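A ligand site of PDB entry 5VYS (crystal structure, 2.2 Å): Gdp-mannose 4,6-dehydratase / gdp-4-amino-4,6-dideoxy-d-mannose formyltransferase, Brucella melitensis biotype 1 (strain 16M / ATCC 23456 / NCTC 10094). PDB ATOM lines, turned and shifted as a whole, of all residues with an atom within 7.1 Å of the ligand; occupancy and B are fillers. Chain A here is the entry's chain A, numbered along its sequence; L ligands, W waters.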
ATOM      1  N   SER A  86      -0.118 -18.344 -29.782  1.00  0.00           N
ATOM      2  CA  SER A  86      -0.548 -19.136 -28.649  1.00  0.00           C
ATOM      3  C   SER A  86       0.175 -18.699 -27.367  1.00  0.00           C
ATOM      4  O   SER A  86       1.393 -18.898 -27.219  1.00  0.00           O
ATOM      5  CB  SER A  86      -0.340 -20.629 -28.918  1.00  0.00           C
ATOM      6  OG  SER A  86      -0.564 -21.402 -27.715  1.00  0.00           O
ATOM      7  N   HIS A  88      -0.032 -19.492 -23.615  1.00  0.00           N
ATOM      8  CA  HIS A  88      -0.480 -20.472 -22.606  1.00  0.00           C
ATOM      9  C   HIS A  88      -1.823 -21.096 -22.922  1.00  0.00           C
ATOM     10  O   HIS A  88      -2.530 -21.529 -22.003  1.00  0.00           O
ATOM     11  CB  HIS A  88      -0.513 -19.872 -21.204  1.00  0.00           C
ATOM     12  CG  HIS A  88       0.830 -19.545 -20.631  1.00  0.00           C
ATOM     13  ND1 HIS A  88       1.023 -19.335 -19.292  1.00  0.00           N
ATOM     14  CD2 HIS A  88       2.040 -19.411 -21.217  1.00  0.00           C
ATOM     15  CE1 HIS A  88       2.293 -19.075 -19.077  1.00  0.00           C
ATOM     16  NE2 HIS A  88       2.933 -19.107 -20.228  1.00  0.00           N
ATOM     17  N   TYR A  89      -2.170 -21.192 -24.205  1.00  0.00           N
ATOM     18  CA  TYR A  89      -3.325 -22.011 -24.614  1.00  0.00           C
ATOM     19  C   TYR A  89      -3.035 -23.422 -24.134  1.00  0.00           C
ATOM     20  O   TYR A  89      -1.928 -23.860 -24.242  1.00  0.00           O
ATOM     21  CB  TYR A  89      -3.519 -21.956 -26.139  1.00  0.00           C
ATOM     22  CG  TYR A  89      -4.887 -22.435 -26.564  1.00  0.00           C
ATOM     23  CD1 TYR A  89      -6.015 -21.706 -26.266  1.00  0.00           C
ATOM     24  CD2 TYR A  89      -5.035 -23.612 -27.227  1.00  0.00           C
ATOM     25  CE1 TYR A  89      -7.281 -22.140 -26.625  1.00  0.00           C
ATOM     26  CE2 TYR A  89      -6.305 -24.060 -27.604  1.00  0.00           C
ATOM     27  CZ  TYR A  89      -7.432 -23.319 -27.298  1.00  0.00           C
ATOM     28  OH  TYR A  89      -8.679 -23.779 -27.648  1.00  0.00           O
ATOM     29  N   ARG A  90      -4.028 -24.136 -23.620  1.00  0.00           N
ATOM     30  CA  ARG A  90      -3.799 -25.427 -22.911  1.00  0.00           C
ATOM     31  C   ARG A  90      -4.245 -26.636 -23.729  1.00  0.00           C
ATOM     32  O   ARG A  90      -4.278 -27.735 -23.192  1.00  0.00           O
ATOM     33  CB  ARG A  90      -4.551 -25.488 -21.554  1.00  0.00           C
ATOM     34  CG  ARG A  90      -4.209 -24.429 -20.510  1.00  0.00           C
ATOM     35  CD  ARG A  90      -5.163 -24.480 -19.316  1.00  0.00           C
ATOM     36  NE  ARG A  90      -4.821 -25.557 -18.389  1.00  0.00           N
ATOM     37  CZ  ARG A  90      -3.798 -25.517 -17.513  1.00  0.00           C
ATOM     38  NH1 ARG A  90      -3.000 -24.443 -17.410  1.00  0.00           N
ATOM     39  NH2 ARG A  90      -3.579 -26.572 -16.733  1.00  0.00           N
ATOM     40  N   SER A  91      -4.664 -26.463 -24.973  1.00  0.00           N
ATOM     41  CA  SER A  91      -5.031 -27.585 -25.824  1.00  0.00           C
ATOM     42  C   SER A  91      -4.163 -27.658 -27.082  1.00  0.00           C
ATOM     43  O   SER A  91      -3.553 -26.663 -27.513  1.00  0.00           O
ATOM     44  CB  SER A  91      -6.502 -27.505 -26.230  1.00  0.00           C
ATOM     45  OG  SER A  91      -7.353 -27.251 -25.124  1.00  0.00           O
ATOM     46  N   LEU A  92      -4.117 -28.849 -27.664  1.00  0.00           N
ATOM     47  CA  LEU A  92      -3.551 -28.984 -28.984  1.00  0.00           C
ATOM     48  C   LEU A  92      -4.454 -28.285 -29.993  1.00  0.00           C
ATOM     49  O   LEU A  92      -5.664 -28.464 -30.030  1.00  0.00           O
ATOM     50  CB  LEU A  92      -3.389 -30.433 -29.387  1.00  0.00           C
ATOM     51  CG  LEU A  92      -2.491 -30.598 -30.613  1.00  0.00           C
ATOM     52  CD1 LEU A  92      -0.991 -30.357 -30.339  1.00  0.00           C
ATOM     53  CD2 LEU A  92      -2.714 -32.006 -31.159  1.00  0.00           C
ATOM     54  N   ILE A  93      -3.824 -27.499 -30.846  1.00  0.00           N
ATOM     55  CA  ILE A  93      -4.529 -26.728 -31.838  1.00  0.00           C
ATOM     56  C   ILE A  93      -4.415 -27.572 -33.117  1.00  0.00           C
ATOM     57  O   ILE A  93      -3.290 -27.921 -33.518  1.00  0.00           O
ATOM     58  CB  ILE A  93      -3.901 -25.343 -32.037  1.00  0.00           C
ATOM     59  CG1 ILE A  93      -4.118 -24.495 -30.769  1.00  0.00           C
ATOM     60  CG2 ILE A  93      -4.498 -24.665 -33.290  1.00  0.00           C
ATOM     61  CD1 ILE A  93      -3.219 -23.288 -30.705  1.00  0.00           C
ATOM     62  N   PRO A  94      -5.538 -27.922 -33.723  1.00  0.00           N
ATOM     63  CA  PRO A  94      -5.463 -28.790 -34.888  1.00  0.00           C
ATOM     64  C   PRO A  94      -4.672 -28.149 -36.029  1.00  0.00           C
ATOM     65  O   PRO A  94      -4.718 -26.910 -36.228  1.00  0.00           O
ATOM     66  CB  PRO A  94      -6.913 -28.957 -35.311  1.00  0.00           C
ATOM     67  CG  PRO A  94      -7.730 -28.545 -34.175  1.00  0.00           C
ATOM     68  CD  PRO A  94      -6.926 -27.528 -33.430  1.00  0.00           C
ATOM     69  N   GLY A  95      -3.987 -28.998 -36.782  1.00  0.00           N
ATOM     70  CA  GLY A  95      -3.259 -28.595 -37.958  1.00  0.00           C
ATOM     71  C   GLY A  95      -4.078 -27.752 -38.897  1.00  0.00           C
ATOM     72  O   GLY A  95      -3.580 -26.753 -39.400  1.00  0.00           O
ATOM     73  N   LEU A  98      -4.230 -24.117 -37.726  1.00  0.00           N
ATOM     74  CA  LEU A  98      -2.977 -23.441 -37.929  1.00  0.00           C
ATOM     75  C   LEU A  98      -2.798 -23.066 -39.385  1.00  0.00           C
ATOM     76  O   LEU A  98      -2.445 -21.950 -39.684  1.00  0.00           O
ATOM     77  CB  LEU A  98      -1.830 -24.315 -37.506  1.00  0.00           C
ATOM     78  CG  LEU A  98      -1.774 -24.594 -36.006  1.00  0.00           C
ATOM     79  CD1 LEU A  98      -0.704 -25.650 -35.776  1.00  0.00           C
ATOM     80  CD2 LEU A  98      -1.509 -23.323 -35.240  1.00  0.00           C
ATOM     81  N   SER A 105       2.341 -19.375 -37.094  1.00  0.00           N
ATOM     82  CA  SER A 105       1.985 -19.245 -35.734  1.00  0.00           C
ATOM     83  C   SER A 105       3.190 -19.175 -34.815  1.00  0.00           C
ATOM     84  O   SER A 105       4.306 -19.474 -35.213  1.00  0.00           O
ATOM     85  CB  SER A 105       1.069 -20.408 -35.373  1.00  0.00           C
ATOM     86  OG  SER A 105       1.784 -21.611 -35.277  1.00  0.00           O
ATOM     87  N   ASN A 107       4.133 -20.102 -30.468  1.00  0.00           N
ATOM     88  CA  ASN A 107       3.725 -20.539 -29.140  1.00  0.00           C
ATOM     89  C   ASN A 107       4.816 -20.248 -28.147  1.00  0.00           C
ATOM     90  O   ASN A 107       5.996 -20.378 -28.485  1.00  0.00           O
ATOM     91  CB  ASN A 107       3.394 -22.023 -29.132  1.00  0.00           C
ATOM     92  CG  ASN A 107       3.141 -22.569 -27.734  1.00  0.00           C
ATOM     93  OD1 ASN A 107       3.977 -23.315 -27.175  1.00  0.00           O
ATOM     94  ND2 ASN A 107       2.034 -22.179 -27.144  1.00  0.00           N
ATOM     95  N   LEU A 108       4.412 -19.841 -26.949  1.00  0.00           N
ATOM     96  CA  LEU A 108       5.331 -19.647 -25.826  1.00  0.00           C
ATOM     97  C   LEU A 108       5.423 -20.910 -24.973  1.00  0.00           C
ATOM     98  O   LEU A 108       4.490 -21.267 -24.309  1.00  0.00           O
ATOM     99  CB  LEU A 108       4.851 -18.526 -24.897  1.00  0.00           C
ATOM    100  CG  LEU A 108       5.662 -18.357 -23.607  1.00  0.00           C
ATOM    101  CD1 LEU A 108       7.146 -18.220 -23.916  1.00  0.00           C
ATOM    102  CD2 LEU A 108       5.175 -17.155 -22.832  1.00  0.00           C
ATOM    103  N   HIS A 109       6.590 -21.557 -24.969  1.00  0.00           N
ATOM    104  CA  HIS A 109       6.835 -22.697 -24.105  1.00  0.00           C
ATOM    105  C   HIS A 109       7.889 -22.317 -23.076  1.00  0.00           C
ATOM    106  O   HIS A 109       8.945 -21.849 -23.460  1.00  0.00           O
ATOM    107  CB  HIS A 109       7.346 -23.867 -24.915  1.00  0.00           C
ATOM    108  CG  HIS A 109       7.460 -25.100 -24.106  1.00  0.00           C
ATOM    109  ND1 HIS A 109       6.355 -25.787 -23.649  1.00  0.00           N
ATOM    110  CD2 HIS A 109       8.532 -25.695 -23.559  1.00  0.00           C
ATOM    111  CE1 HIS A 109       6.759 -26.790 -22.897  1.00  0.00           C
ATOM    112  NE2 HIS A 109       8.077 -26.755 -22.821  1.00  0.00           N
ATOM    113  N   LEU A 113      13.593 -25.515 -25.436  1.00  0.00           N
ATOM    114  CA  LEU A 113      13.224 -26.684 -26.256  1.00  0.00           C
ATOM    115  C   LEU A 113      14.403 -27.086 -27.134  1.00  0.00           C
ATOM    116  O   LEU A 113      15.184 -26.221 -27.462  1.00  0.00           O
ATOM    117  CB  LEU A 113      11.997 -26.378 -27.120  1.00  0.00           C
ATOM    118  CG  LEU A 113      10.650 -26.221 -26.424  1.00  0.00           C
ATOM    119  CD1 LEU A 113       9.677 -25.552 -27.373  1.00  0.00           C
ATOM    120  CD2 LEU A 113      10.126 -27.539 -25.930  1.00  0.00           C
ATOM    121  N   HIS A 138       8.252 -20.503 -30.270  1.00  0.00           N
ATOM    122  CA  HIS A 138       8.432 -21.418 -31.437  1.00  0.00           C
ATOM    123  C   HIS A 138       7.218 -21.583 -32.343  1.00  0.00           C
ATOM    124  O   HIS A 138       6.087 -21.695 -31.883  1.00  0.00           O
ATOM    125  CB  HIS A 138       8.833 -22.832 -30.949  1.00  0.00           C
ATOM    126  CG  HIS A 138       7.731 -23.590 -30.252  1.00  0.00           C
ATOM    127  ND1 HIS A 138       6.922 -24.483 -30.915  1.00  0.00           N
ATOM    128  CD2 HIS A 138       7.289 -23.555 -28.972  1.00  0.00           C
ATOM    129  CE1 HIS A 138       6.036 -24.981 -30.075  1.00  0.00           C
ATOM    130  NE2 HIS A 138       6.240 -24.436 -28.886  1.00  0.00           N
ATOM    131  N   ARG A 139       7.466 -21.688 -33.632  1.00  0.00           N
ATOM    132  CA  ARG A 139       6.381 -21.919 -34.575  1.00  0.00           C
ATOM    133  C   ARG A 139       5.748 -23.229 -34.198  1.00  0.00           C
ATOM    134  O   ARG A 139       6.442 -24.156 -33.801  1.00  0.00           O
ATOM    135  CB  ARG A 139       6.883 -21.911 -36.023  1.00  0.00           C
ATOM    136  CG  ARG A 139       7.500 -20.582 -36.464  1.00  0.00           C
ATOM    137  CD  ARG A 139       7.889 -20.566 -37.952  1.00  0.00           C
ATOM    138  NE  ARG A 139       8.163 -19.200 -38.484  1.00  0.00           N
ATOM    139  CZ  ARG A 139       7.251 -18.378 -39.035  1.00  0.00           C
ATOM    140  NH1 ARG A 139       7.619 -17.148 -39.440  1.00  0.00           N
ATOM    141  NH2 ARG A 139       5.962 -18.754 -39.154  1.00  0.00           N
ATOM    142  N   MET A 140       4.431 -23.280 -34.249  1.00  0.00           N
ATOM    143  CA  MET A 140       3.724 -24.528 -34.044  1.00  0.00           C
ATOM    144  C   MET A 140       3.549 -25.321 -35.349  1.00  0.00           C
ATOM    145  O   MET A 140       3.236 -24.778 -36.427  1.00  0.00           O
ATOM    146  CB  MET A 140       2.359 -24.282 -33.437  1.00  0.00           C
ATOM    147  CG  MET A 140       2.410 -23.566 -32.097  1.00  0.00           C
ATOM    148  SD  MET A 140       0.760 -23.374 -31.441  1.00  0.00           S
ATOM    149  CE  MET A 140       0.259 -21.889 -32.287  1.00  0.00           C
ATOM    150  N   ASP A 141       3.740 -26.626 -35.203  1.00  0.00           N
ATOM    151  CA  ASP A 141       3.302 -27.645 -36.162  1.00  0.00           C
ATOM    152  C   ASP A 141       2.129 -28.435 -35.499  1.00  0.00           C
ATOM    153  O   ASP A 141       1.567 -27.958 -34.491  1.00  0.00           O
ATOM    154  CB  ASP A 141       4.492 -28.556 -36.537  1.00  0.00           C
ATOM    155  CG  ASP A 141       5.165 -29.212 -35.335  1.00  0.00           C
ATOM    156  OD1 ASP A 141       4.464 -29.618 -34.381  1.00  0.00           O
ATOM    157  OD2 ASP A 141       6.399 -29.323 -35.330  1.00  0.00           O
ATOM    158  N   GLU A 142       1.770 -29.615 -36.030  1.00  0.00           N
ATOM    159  CA  GLU A 142       0.580 -30.350 -35.535  1.00  0.00           C
ATOM    160  C   GLU A 142       0.807 -31.077 -34.197  1.00  0.00           C
ATOM    161  O   GLU A 142      -0.149 -31.548 -33.565  1.00  0.00           O
ATOM    162  CB  GLU A 142      -0.009 -31.308 -36.609  1.00  0.00           C
ATOM    163  CG  GLU A 142       0.883 -32.472 -37.081  1.00  0.00           C
ATOM    164  CD  GLU A 142       1.916 -32.082 -38.137  1.00  0.00           C
ATOM    165  OE1 GLU A 142       1.959 -30.894 -38.568  1.00  0.00           O
ATOM    166  OE2 GLU A 142       2.713 -32.969 -38.543  1.00  0.00           O
ATOM    167  N   ASN A 143       2.068 -31.177 -33.784  1.00  0.00           N
ATOM    168  CA  ASN A 143       2.467 -31.774 -32.496  1.00  0.00           C
ATOM    169  C   ASN A 143       2.754 -30.714 -31.424  1.00  0.00           C
ATOM    170  O   ASN A 143       2.953 -29.548 -31.761  1.00  0.00           O
ATOM    171  CB  ASN A 143       3.692 -32.669 -32.737  1.00  0.00           C
ATOM    172  CG  ASN A 143       3.437 -33.738 -33.785  1.00  0.00           C
ATOM    173  OD1 ASN A 143       2.471 -34.483 -33.692  1.00  0.00           O
ATOM    174  ND2 ASN A 143       4.285 -33.785 -34.817  1.00  0.00           N
ATOM    175  N   PHE A 144       2.716 -31.111 -30.158  1.00  0.00           N
ATOM    176  CA  PHE A 144       3.169 -30.235 -29.056  1.00  0.00           C
ATOM    177  C   PHE A 144       4.701 -30.059 -29.089  1.00  0.00           C
ATOM    178  O   PHE A 144       5.431 -31.071 -29.146  1.00  0.00           O
ATOM    179  CB  PHE A 144       2.798 -30.790 -27.660  1.00  0.00           C
ATOM    180  CG  PHE A 144       1.387 -30.473 -27.204  1.00  0.00           C
ATOM    181  CD1 PHE A 144       1.037 -29.174 -26.805  1.00  0.00           C
ATOM    182  CD2 PHE A 144       0.426 -31.477 -27.120  1.00  0.00           C
ATOM    183  CE1 PHE A 144      -0.247 -28.858 -26.357  1.00  0.00           C
ATOM    184  CE2 PHE A 144      -0.859 -31.173 -26.680  1.00  0.00           C
ATOM    185  CZ  PHE A 144      -1.202 -29.863 -26.285  1.00  0.00           C
ATOM    186  N   ASP A 145       5.157 -28.799 -29.056  1.00  0.00           N
ATOM    187  CA  ASP A 145       6.508 -28.422 -28.583  1.00  0.00           C
ATOM    188  C   ASP A 145       7.645 -28.732 -29.554  1.00  0.00           C
ATOM    189  O   ASP A 145       8.819 -28.689 -29.155  1.00  0.00           O
ATOM    190  CB  ASP A 145       6.865 -29.095 -27.244  1.00  0.00           C
ATOM    191  CG  ASP A 145       5.788 -28.987 -26.185  1.00  0.00           C
ATOM    192  OD1 ASP A 145       5.216 -27.901 -25.947  1.00  0.00           O
ATOM    193  OD2 ASP A 145       5.553 -30.006 -25.536  1.00  0.00           O
ATOM    194  N   THR A 146       7.315 -29.027 -30.810  1.00  0.00           N
ATOM    195  CA  THR A 146       8.267 -29.542 -31.806  1.00  0.00           C
ATOM    196  C   THR A 146       8.677 -28.572 -32.896  1.00  0.00           C
ATOM    197  O   THR A 146       9.722 -28.775 -33.528  1.00  0.00           O
ATOM    198  CB  THR A 146       7.681 -30.778 -32.488  1.00  0.00           C
ATOM    199  OG1 THR A 146       6.294 -30.557 -32.704  1.00  0.00           O
ATOM    200  CG2 THR A 146       7.857 -31.992 -31.585  1.00  0.00           C
ATOM    201  N   GLY A 147       7.913 -27.513 -33.117  1.00  0.00           N
ATOM    202  CA  GLY A 147       8.216 -26.616 -34.243  1.00  0.00           C
ATOM    203  C   GLY A 147       9.446 -25.731 -34.097  1.00  0.00           C
ATOM    204  O   GLY A 147      10.086 -25.724 -33.070  1.00  0.00           O
HETATM  205  N1  LIG L   1       1.449 -27.253 -31.262  1.00  0.00           N
HETATM  206  C1  LIG L   1       0.097 -27.204 -31.356  1.00  0.00           C
HETATM  207  N2  LIG L   1      -0.658 -26.710 -30.333  1.00  0.00           N
HETATM  208  C2  LIG L   1      -0.149 -26.249 -29.180  1.00  0.00           C
HETATM  209  C3  LIG L   1       1.304 -26.289 -28.981  1.00  0.00           C
HETATM  210  C4  LIG L   1       2.080 -26.830 -30.151  1.00  0.00           C
HETATM  211  N3  LIG L   1      -0.930 -25.797 -28.193  1.00  0.00           N
HETATM  212  C5  LIG L   1      -0.428 -25.356 -27.012  1.00  0.00           C
HETATM  213  C6  LIG L   1       1.016 -25.346 -26.660  1.00  0.00           C
HETATM  214  N4  LIG L   1       1.859 -25.819 -27.759  1.00  0.00           N
HETATM  215  O1  LIG L   1       3.339 -26.888 -30.111  1.00  0.00           O
HETATM  216  N5  LIG L   1      -0.460 -27.645 -32.508  1.00  0.00           N
HETATM  217  O   HOH W   1       5.275 -27.264 -32.469  1.00  0.00           O
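The backbone carbonyl oxygen (O) of Ile 93 is in hydrogen-bond range of a nitrogen (N5) of the ligand (3.0 Å). The backbone NH (N) of Asp 145 lies within hydrogen-bond range of an oxygen (O1) of the ligand. N of Ile 93 lies within hydrogen-bond range of N2 of the ligand. A nitrogen (N4) of the ligand is in hydrogen-bond range of the side-chain amide oxygen of Asn 107. The backbone carbonyl oxygen (O) of Asp 141 sits at hydrogen-bond distance from a nitrogen (N5) of the ligand (2.9 Å). The backbone carbonyl oxygen (O) of Asn 143 sits at hydrogen-bond distance from a nitrogen (N1) of the ligand (2.8 Å). The backbone carbonyl oxygen of Ser 91 lies within hydrogen-bond range of a nitrogen (N3) of the ligand, at 2.8 Å.
The side-chain sulfur (SD) of Met 140 sits close to a nitrogen (N2) of the ligand (3.8 Å). Tyr 89 touches the ligand. CD1 of Leu 92 touches C1 of the ligand, 3.5 Å away. Leu 98 touches the ligand (CD1 to N5, 3.8 Å). CE1 of His 138 touches O1 of the ligand, 3.3 Å away. Phe 144 touches the ligand (CA to O1, 3.5 Å). Hydrophobic or aromatic side chains within 4 Å of the ligand: Leu 92, Ile 93, Leu 98, His 138, Met 140 and Phe 144. Within 4 Å of the ligand: Tyr 89, Ser 91, Leu 92, Ile 93, Leu 98, Asn 107, His 138, Met 140, Asp 141, Asn 143, Phe 144 and Asp 145.
The backbone NH (N) of Met 140 lies within hydrogen-bond range of the side-chain hydroxyl (OG) of Ser 105. The backbone NH (N) of Gly 147 lies within hydrogen-bond range of the side-chain carboxylate (OD2) of Asp 141 (3.2 Å). The backbone NH (N) of Asn 143 lies within hydrogen-bond range of the side-chain carboxylate (OD1) of Asp 141 (2.9 Å). The backbone carbonyl oxygen (O) of Asn 107 is in hydrogen-bond range of the backbone NH (N) of His 138 (2.9 Å). The side-chain hydroxyl (OG1) of Thr 146 is in hydrogen-bond range of the side-chain carboxylate (OD1) of Asp 141 (2.7 Å). The side-chain carboxylate (OD1) of Asp 145 is in hydrogen-bond range of a ring nitrogen (ND1) of His 109 (3.3 Å). ND2 of Asn 107 lies within hydrogen-bond range of OG of Ser 86 (2.8 Å).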
